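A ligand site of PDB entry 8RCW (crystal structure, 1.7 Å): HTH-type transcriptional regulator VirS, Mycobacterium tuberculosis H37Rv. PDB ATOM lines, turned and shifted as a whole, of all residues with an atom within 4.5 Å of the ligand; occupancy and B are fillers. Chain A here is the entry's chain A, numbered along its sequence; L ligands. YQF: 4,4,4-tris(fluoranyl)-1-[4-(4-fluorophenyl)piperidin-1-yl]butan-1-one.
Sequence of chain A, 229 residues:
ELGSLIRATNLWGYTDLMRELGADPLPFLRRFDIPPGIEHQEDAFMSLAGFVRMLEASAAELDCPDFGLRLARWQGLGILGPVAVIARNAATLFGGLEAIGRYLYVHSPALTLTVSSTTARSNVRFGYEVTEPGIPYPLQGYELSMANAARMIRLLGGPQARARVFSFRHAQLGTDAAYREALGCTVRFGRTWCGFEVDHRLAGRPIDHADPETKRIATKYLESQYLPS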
ATOM      1  N   ILE A   6      11.862 -26.239  29.736  1.00  0.00           N
ATOM      2  CA  ILE A   6      12.920 -26.823  28.920  1.00  0.00           C
ATOM      3  C   ILE A   6      13.380 -28.136  29.546  1.00  0.00           C
ATOM      4  O   ILE A   6      13.350 -28.299  30.767  1.00  0.00           O
ATOM      5  CB  ILE A   6      14.060 -25.799  28.732  1.00  0.00           C
ATOM      6  CG1 ILE A   6      15.154 -26.296  27.782  1.00  0.00           C
ATOM      7  CG2 ILE A   6      14.673 -25.404  30.071  1.00  0.00           C
ATOM      8  CD1 ILE A   6      16.048 -25.164  27.284  1.00  0.00           C
ATOM      9  N   ASN A  10      19.420 -29.761  30.041  1.00  0.00           N
ATOM     10  CA  ASN A  10      20.112 -28.515  29.760  1.00  0.00           C
ATOM     11  C   ASN A  10      20.820 -28.004  31.003  1.00  0.00           C
ATOM     12  O   ASN A  10      21.559 -27.037  30.912  1.00  0.00           O
ATOM     13  CB  ASN A  10      19.160 -27.515  29.101  1.00  0.00           C
ATOM     14  CG  ASN A  10      19.729 -26.935  27.823  1.00  0.00           C
ATOM     15  OD1 ASN A  10      19.083 -26.865  26.796  1.00  0.00           O
ATOM     16  ND2 ASN A  10      20.945 -26.462  27.917  1.00  0.00           N
ATOM     17  N   LEU A  48      12.158 -22.568  31.922  1.00  0.00           N
ATOM     18  CA  LEU A  48      13.147 -21.950  31.042  1.00  0.00           C
ATOM     19  C   LEU A  48      13.537 -20.559  31.588  1.00  0.00           C
ATOM     20  O   LEU A  48      14.726 -20.243  31.630  1.00  0.00           O
ATOM     21  CB  LEU A  48      12.610 -21.821  29.626  1.00  0.00           C
ATOM     22  CG  LEU A  48      13.511 -21.047  28.643  1.00  0.00           C
ATOM     23  CD1 LEU A  48      14.875 -21.720  28.471  1.00  0.00           C
ATOM     24  CD2 LEU A  48      12.820 -20.946  27.329  1.00  0.00           C
ATOM     25  N   PHE A  51      15.839 -21.014  34.506  1.00  0.00           N
ATOM     26  CA  PHE A  51      17.124 -21.513  34.077  1.00  0.00           C
ATOM     27  C   PHE A  51      17.954 -20.356  33.499  1.00  0.00           C
ATOM     28  O   PHE A  51      19.119 -20.205  33.859  1.00  0.00           O
ATOM     29  CB  PHE A  51      16.906 -22.658  33.097  1.00  0.00           C
ATOM     30  CG  PHE A  51      18.195 -23.143  32.463  1.00  0.00           C
ATOM     31  CD1 PHE A  51      19.224 -23.624  33.273  1.00  0.00           C
ATOM     32  CD2 PHE A  51      18.376 -23.092  31.091  1.00  0.00           C
ATOM     33  CE1 PHE A  51      20.386 -24.094  32.694  1.00  0.00           C
ATOM     34  CE2 PHE A  51      19.549 -23.551  30.527  1.00  0.00           C
ATOM     35  CZ  PHE A  51      20.537 -24.071  31.327  1.00  0.00           C
ATOM     36  N   VAL A  52      17.376 -19.579  32.593  1.00  0.00           N
ATOM     37  CA  VAL A  52      18.166 -18.528  31.955  1.00  0.00           C
ATOM     38  C   VAL A  52      18.553 -17.449  32.973  1.00  0.00           C
ATOM     39  O   VAL A  52      19.655 -16.925  32.905  1.00  0.00           O
ATOM     40  CB  VAL A  52      17.530 -17.903  30.700  1.00  0.00           C
ATOM     41  CG1 VAL A  52      17.275 -18.898  29.594  1.00  0.00           C
ATOM     42  CG2 VAL A  52      16.272 -17.163  30.969  1.00  0.00           C
ATOM     43  N   LEU A  55      21.520 -18.819  34.960  1.00  0.00           N
ATOM     44  CA  LEU A  55      22.776 -18.754  34.242  1.00  0.00           C
ATOM     45  C   LEU A  55      23.359 -17.354  34.379  1.00  0.00           C
ATOM     46  O   LEU A  55      24.562 -17.213  34.545  1.00  0.00           O
ATOM     47  CB  LEU A  55      22.567 -19.076  32.757  1.00  0.00           C
ATOM     48  CG  LEU A  55      22.287 -20.524  32.408  1.00  0.00           C
ATOM     49  CD1 LEU A  55      22.046 -20.687  30.918  1.00  0.00           C
ATOM     50  CD2 LEU A  55      23.398 -21.404  32.890  1.00  0.00           C
ATOM     51  N   GLN A  75      27.573 -31.276  28.121  1.00  0.00           N
ATOM     52  CA  GLN A  75      26.278 -31.375  27.471  1.00  0.00           C
ATOM     53  C   GLN A  75      26.424 -32.013  26.071  1.00  0.00           C
ATOM     54  O   GLN A  75      26.675 -33.194  25.977  1.00  0.00           O
ATOM     55  CB  GLN A  75      25.597 -30.013  27.504  1.00  0.00           C
ATOM     56  CG  GLN A  75      25.346 -29.540  28.947  1.00  0.00           C
ATOM     57  CD  GLN A  75      24.371 -28.407  29.092  1.00  0.00           C
ATOM     58  OE1 GLN A  75      23.812 -27.886  28.116  1.00  0.00           O
ATOM     59  NE2 GLN A  75      24.167 -28.005  30.341  1.00  0.00           N
ATOM     60  N   ILE A  79      21.879 -34.006  25.272  1.00  0.00           N
ATOM     61  CA  ILE A  79      20.867 -33.256  25.990  1.00  0.00           C
ATOM     62  C   ILE A  79      19.554 -33.192  25.236  1.00  0.00           C
ATOM     63  O   ILE A  79      18.525 -32.904  25.878  1.00  0.00           O
ATOM     64  CB  ILE A  79      21.305 -31.855  26.457  1.00  0.00           C
ATOM     65  CG1 ILE A  79      21.414 -30.853  25.314  1.00  0.00           C
ATOM     66  CG2 ILE A  79      22.597 -31.950  27.265  1.00  0.00           C
ATOM     67  CD1 ILE A  79      21.418 -29.403  25.784  1.00  0.00           C
ATOM     68  N   ILE A 100      16.505 -31.547  14.127  1.00  0.00           N
ATOM     69  CA  ILE A 100      16.549 -30.848  15.386  1.00  0.00           C
ATOM     70  C   ILE A 100      15.663 -29.605  15.298  1.00  0.00           C
ATOM     71  O   ILE A 100      14.891 -29.326  16.224  1.00  0.00           O
ATOM     72  CB  ILE A 100      17.972 -30.561  15.839  1.00  0.00           C
ATOM     73  CG1 ILE A 100      18.750 -31.839  16.097  1.00  0.00           C
ATOM     74  CG2 ILE A 100      17.970 -29.616  17.025  1.00  0.00           C
ATOM     75  CD1 ILE A 100      20.250 -31.629  16.297  1.00  0.00           C
ATOM     76  N   LEU A 104      12.417 -28.928  17.649  1.00  0.00           N
ATOM     77  CA  LEU A 104      13.079 -28.291  18.778  1.00  0.00           C
ATOM     78  C   LEU A 104      12.089 -27.921  19.897  1.00  0.00           C
ATOM     79  O   LEU A 104      12.480 -27.842  21.075  1.00  0.00           O
ATOM     80  CB  LEU A 104      13.846 -27.055  18.281  1.00  0.00           C
ATOM     81  CG  LEU A 104      14.795 -26.430  19.308  1.00  0.00           C
ATOM     82  CD1 LEU A 104      15.789 -27.426  19.838  1.00  0.00           C
ATOM     83  CD2 LEU A 104      15.531 -25.248  18.678  1.00  0.00           C
ATOM     84  N   HIS A 107      12.217 -29.996  22.928  1.00  0.00           N
ATOM     85  CA  HIS A 107      13.206 -29.593  23.902  1.00  0.00           C
ATOM     86  C   HIS A 107      12.661 -28.455  24.768  1.00  0.00           C
ATOM     87  O   HIS A 107      12.767 -28.492  25.992  1.00  0.00           O
ATOM     88  CB  HIS A 107      14.517 -29.215  23.187  1.00  0.00           C
ATOM     89  CG  HIS A 107      15.654 -29.096  24.149  1.00  0.00           C
ATOM     90  ND1 HIS A 107      16.204 -30.207  24.743  1.00  0.00           N
ATOM     91  CD2 HIS A 107      16.321 -28.065  24.636  1.00  0.00           C
ATOM     92  CE1 HIS A 107      17.206 -29.803  25.547  1.00  0.00           C
ATOM     93  NE2 HIS A 107      17.251 -28.496  25.525  1.00  0.00           N
ATOM     94  N   LEU A 111      12.119 -22.210  21.961  1.00  0.00           N
ATOM     95  CA  LEU A 111      13.286 -22.171  21.094  1.00  0.00           C
ATOM     96  C   LEU A 111      12.836 -22.339  19.659  1.00  0.00           C
ATOM     97  O   LEU A 111      12.102 -23.272  19.355  1.00  0.00           O
ATOM     98  CB  LEU A 111      14.223 -23.290  21.485  1.00  0.00           C
ATOM     99  CG  LEU A 111      14.684 -23.288  22.944  1.00  0.00           C
ATOM    100  CD1 LEU A 111      15.627 -24.431  23.191  1.00  0.00           C
ATOM    101  CD2 LEU A 111      15.299 -21.984  23.376  1.00  0.00           C
ATOM    102  N   LEU A 113      14.493 -22.574  15.699  1.00  0.00           N
ATOM    103  CA  LEU A 113      15.576 -22.670  14.748  1.00  0.00           C
ATOM    104  C   LEU A 113      15.000 -22.499  13.338  1.00  0.00           C
ATOM    105  O   LEU A 113      14.036 -23.176  12.932  1.00  0.00           O
ATOM    106  CB  LEU A 113      16.228 -24.026  14.874  1.00  0.00           C
ATOM    107  CG  LEU A 113      17.553 -24.181  14.145  1.00  0.00           C
ATOM    108  CD1 LEU A 113      18.632 -23.319  14.809  1.00  0.00           C
ATOM    109  CD2 LEU A 113      17.992 -25.623  14.111  1.00  0.00           C
ATOM    110  N   PHE A 126      21.733 -21.429  10.091  1.00  0.00           N
ATOM    111  CA  PHE A 126      20.976 -21.955  11.209  1.00  0.00           C
ATOM    112  C   PHE A 126      20.748 -20.803  12.181  1.00  0.00           C
ATOM    113  O   PHE A 126      21.618 -20.451  12.969  1.00  0.00           O
ATOM    114  CB  PHE A 126      21.704 -23.142  11.848  1.00  0.00           C
ATOM    115  CG  PHE A 126      21.778 -24.317  10.934  1.00  0.00           C
ATOM    116  CD1 PHE A 126      22.744 -24.377   9.955  1.00  0.00           C
ATOM    117  CD2 PHE A 126      20.808 -25.292  10.959  1.00  0.00           C
ATOM    118  CE1 PHE A 126      22.799 -25.448   9.089  1.00  0.00           C
ATOM    119  CE2 PHE A 126      20.859 -26.374  10.099  1.00  0.00           C
ATOM    120  CZ  PHE A 126      21.846 -26.430   9.127  1.00  0.00           C
ATOM    121  N   TYR A 128      18.874 -18.940  15.258  1.00  0.00           N
ATOM    122  CA  TYR A 128      18.348 -19.426  16.523  1.00  0.00           C
ATOM    123  C   TYR A 128      17.823 -18.283  17.382  1.00  0.00           C
ATOM    124  O   TYR A 128      18.508 -17.268  17.582  1.00  0.00           O
ATOM    125  CB  TYR A 128      19.536 -20.081  17.197  1.00  0.00           C
ATOM    126  CG  TYR A 128      19.224 -20.610  18.580  1.00  0.00           C
ATOM    127  CD1 TYR A 128      18.360 -21.689  18.755  1.00  0.00           C
ATOM    128  CD2 TYR A 128      19.829 -20.037  19.690  1.00  0.00           C
ATOM    129  CE1 TYR A 128      18.151 -22.220  20.008  1.00  0.00           C
ATOM    130  CE2 TYR A 128      19.623 -20.579  20.955  1.00  0.00           C
ATOM    131  CZ  TYR A 128      18.815 -21.683  21.105  1.00  0.00           C
ATOM    132  OH  TYR A 128      18.648 -22.235  22.360  1.00  0.00           O
ATOM    133  N   VAL A 130      15.627 -17.505  21.229  1.00  0.00           N
ATOM    134  CA  VAL A 130      14.937 -17.861  22.456  1.00  0.00           C
ATOM    135  C   VAL A 130      13.845 -16.811  22.631  1.00  0.00           C
ATOM    136  O   VAL A 130      14.128 -15.616  22.740  1.00  0.00           O
ATOM    137  CB  VAL A 130      15.899 -17.822  23.664  1.00  0.00           C
ATOM    138  CG1 VAL A 130      15.164 -18.166  24.964  1.00  0.00           C
ATOM    139  CG2 VAL A 130      17.093 -18.719  23.452  1.00  0.00           C
ATOM    140  N   GLY A 141      22.571 -18.096  28.030  1.00  0.00           N
ATOM    141  CA  GLY A 141      21.747 -19.081  27.353  1.00  0.00           C
ATOM    142  C   GLY A 141      22.108 -19.233  25.869  1.00  0.00           C
ATOM    143  O   GLY A 141      22.231 -20.336  25.353  1.00  0.00           O
ATOM    144  N   LEU A 144      25.692 -20.856  25.700  1.00  0.00           N
ATOM    145  CA  LEU A 144      25.544 -22.273  25.927  1.00  0.00           C
ATOM    146  C   LEU A 144      24.928 -22.950  24.700  1.00  0.00           C
ATOM    147  O   LEU A 144      25.404 -24.012  24.307  1.00  0.00           O
ATOM    148  CB  LEU A 144      24.656 -22.471  27.161  1.00  0.00           C
ATOM    149  CG  LEU A 144      24.275 -23.915  27.484  1.00  0.00           C
ATOM    150  CD1 LEU A 144      25.510 -24.770  27.738  1.00  0.00           C
ATOM    151  CD2 LEU A 144      23.367 -23.912  28.740  1.00  0.00           C
ATOM    152  N   SER A 145      23.919 -22.341  24.081  1.00  0.00           N
ATOM    153  CA  SER A 145      23.253 -22.935  22.935  1.00  0.00           C
ATOM    154  C   SER A 145      24.218 -23.173  21.781  1.00  0.00           C
ATOM    155  O   SER A 145      24.264 -24.231  21.151  1.00  0.00           O
ATOM    156  CB  SER A 145      22.125 -22.106  22.491  1.00  0.00           C
ATOM    157  OG  SER A 145      21.136 -21.952  23.508  1.00  0.00           O
ATOM    158  N   MET A 146      25.018 -22.161  21.508  1.00  0.00           N
ATOM    159  CA  MET A 146      25.939 -22.214  20.375  1.00  0.00           C
ATOM    160  C   MET A 146      27.137 -23.125  20.674  1.00  0.00           C
ATOM    161  O   MET A 146      27.568 -23.884  19.786  1.00  0.00           O
ATOM    162  CB  MET A 146      26.402 -20.806  19.989  1.00  0.00           C
ATOM    163  CG  MET A 146      25.319 -19.987  19.372  1.00  0.00           C
ATOM    164  SD  MET A 146      24.480 -20.707  17.948  1.00  0.00           S
ATOM    165  CE  MET A 146      23.003 -21.419  18.690  1.00  0.00           C
ATOM    166  N   ASN A 148      26.932 -25.783  22.537  1.00  0.00           N
ATOM    167  CA  ASN A 148      26.293 -27.074  22.314  1.00  0.00           C
ATOM    168  C   ASN A 148      26.193 -27.367  20.814  1.00  0.00           C
ATOM    169  O   ASN A 148      26.438 -28.491  20.377  1.00  0.00           O
ATOM    170  CB  ASN A 148      24.938 -27.153  23.033  1.00  0.00           C
ATOM    171  CG  ASN A 148      25.110 -27.632  24.465  1.00  0.00           C
ATOM    172  OD1 ASN A 148      26.017 -28.423  24.727  1.00  0.00           O
ATOM    173  ND2 ASN A 148      24.356 -27.100  25.394  1.00  0.00           N
ATOM    174  N   ALA A 149      25.766 -26.369  20.026  1.00  0.00           N
ATOM    175  CA  ALA A 149      25.629 -26.597  18.598  1.00  0.00           C
ATOM    176  C   ALA A 149      26.954 -27.024  17.991  1.00  0.00           C
ATOM    177  O   ALA A 149      26.992 -27.901  17.116  1.00  0.00           O
ATOM    178  CB  ALA A 149      25.064 -25.395  17.907  1.00  0.00           C
ATOM    179  N   MET A 152      27.478 -30.531  18.650  1.00  0.00           N
ATOM    180  CA  MET A 152      26.565 -31.335  17.824  1.00  0.00           C
ATOM    181  C   MET A 152      27.079 -31.453  16.382  1.00  0.00           C
ATOM    182  O   MET A 152      26.941 -32.506  15.764  1.00  0.00           O
ATOM    183  CB  MET A 152      25.155 -30.744  17.796  1.00  0.00           C
ATOM    184  CG  MET A 152      24.458 -30.889  19.159  1.00  0.00           C
ATOM    185  SD  MET A 152      22.959 -29.905  19.310  1.00  0.00           S
ATOM    186  CE  MET A 152      22.689 -30.125  21.080  1.00  0.00           C
ATOM    187  N   PHE A 196      24.595 -20.000  13.402  1.00  0.00           N
ATOM    188  CA  PHE A 196      25.805 -20.372  12.690  1.00  0.00           C
ATOM    189  C   PHE A 196      25.453 -20.733  11.254  1.00  0.00           C
ATOM    190  O   PHE A 196      24.289 -20.861  10.875  1.00  0.00           O
ATOM    191  CB  PHE A 196      26.488 -21.554  13.373  1.00  0.00           C
ATOM    192  CG  PHE A 196      25.651 -22.803  13.459  1.00  0.00           C
ATOM    193  CD1 PHE A 196      25.652 -23.744  12.429  1.00  0.00           C
ATOM    194  CD2 PHE A 196      24.823 -23.010  14.534  1.00  0.00           C
ATOM    195  CE1 PHE A 196      24.850 -24.870  12.505  1.00  0.00           C
ATOM    196  CE2 PHE A 196      23.985 -24.110  14.585  1.00  0.00           C
ATOM    197  CZ  PHE A 196      24.011 -25.059  13.576  1.00  0.00           C
HETATM  198  N1  YQF L   1      20.363 -25.852  23.459  1.00  0.00           N
HETATM  199  C1  YQF L   1      21.290 -26.822  22.856  1.00  0.00           C
HETATM  200  C2  YQF L   1      21.515 -26.534  21.407  1.00  0.00           C
HETATM  201  C3  YQF L   1      20.204 -26.479  20.639  1.00  0.00           C
HETATM  202  C4  YQF L   1      19.269 -25.475  21.288  1.00  0.00           C
HETATM  203  C5  YQF L   1      19.081 -25.796  22.747  1.00  0.00           C
HETATM  204  C6  YQF L   1      20.502 -26.222  19.164  1.00  0.00           C
HETATM  205  C7  YQF L   1      20.664 -27.311  18.321  1.00  0.00           C
HETATM  206  C8  YQF L   1      20.887 -27.137  16.960  1.00  0.00           C
HETATM  207  C9  YQF L   1      21.023 -25.880  16.468  1.00  0.00           C
HETATM  208  C10 YQF L   1      20.912 -24.764  17.270  1.00  0.00           C
HETATM  209  C11 YQF L   1      20.698 -24.946  18.637  1.00  0.00           C
HETATM  210  F1  YQF L   1      21.294 -25.749  15.137  1.00  0.00           F
HETATM  211  C12 YQF L   1      20.670 -25.187  24.586  1.00  0.00           C
HETATM  212  C13 YQF L   1      19.672 -24.197  25.129  1.00  0.00           C
HETATM  213  C14 YQF L   1      20.216 -23.372  26.267  1.00  0.00           C
HETATM  214  C15 YQF L   1      19.251 -22.306  26.667  1.00  0.00           C
HETATM  215  F2  YQF L   1      18.046 -22.735  27.040  1.00  0.00           F
HETATM  216  F3  YQF L   1      18.977 -21.494  25.650  1.00  0.00           F
HETATM  217  F4  YQF L   1      19.730 -21.576  27.669  1.00  0.00           F
HETATM  218  O1  YQF L   1      21.769 -25.301  25.134  1.00  0.00           O
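An oxygen (O1) of the ligand lies within hydrogen-bond range of the side-chain amide nitrogen (ND2) of Asn 10 (3.1 Å). ND2 of Asn 148 sits at hydrogen-bond distance from O1 of the ligand (3.2 Å).
O of Gly 141 sits at hydrogen-bond distance from OG of Ser 145, at 2.7 Å. The side-chain hydroxyl (OG) of Ser 145 is in hydrogen-bond range of the side-chain hydroxyl (OH) of Tyr 128 (2.8 Å). A ring nitrogen (NE2) of His 107 lies within hydrogen-bond range of the side-chain amide oxygen (OD1) of Asn 10 (2.8 Å). The side-chain amide nitrogen (NE2) of Gln 75 is in hydrogen-bond range of the backbone carbonyl oxygen (O) of Asn 10 (2.8 Å). The backbone carbonyl oxygen of Leu 144 sits close to the side-chain amide nitrogen of Asn 148. OE1 of Gln 75 is in hydrogen-bond range of ND2 of Asn 148, at 2.9 Å. N of Phe 126 sits at hydrogen-bond distance from O of Phe 196 (2.7 Å).
A fluorine (F3) of the ligand lies close to the side-chain hydroxyl (OH) of Tyr 128 (3.4 Å). The backbone carbonyl oxygen (O) of Gly 141 lies close to a fluorine (F3) of the ligand, 3.5 Å away. The side-chain hydroxyl (OG) of Ser 145 sits close to a fluorine (F3) of the ligand (3.1 Å). Ile 6 touches the ligand. Leu 48 touches the ligand. Phe 51 touches the ligand. CD1 of Ile 79 touches C1 of the ligand, at 3.9 Å. Ile 100 touches the ligand (CG2 to C7, 3.8 Å). CD1 of Leu 111 touches C5 of the ligand (3.7 Å). Leu 113 touches the ligand. Leu 144 touches the ligand. SD of Met 152 touches C7 of the ligand, at 3.6 Å. Phe 196 touches the ligand. Hydrophobic or aromatic side chains that line the ligand: Ile 6, Leu 48, Phe 51, Ile 79, Ile 100, Leu 111, Leu 113, Tyr 128, Leu 144, Met 152 and Phe 196.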
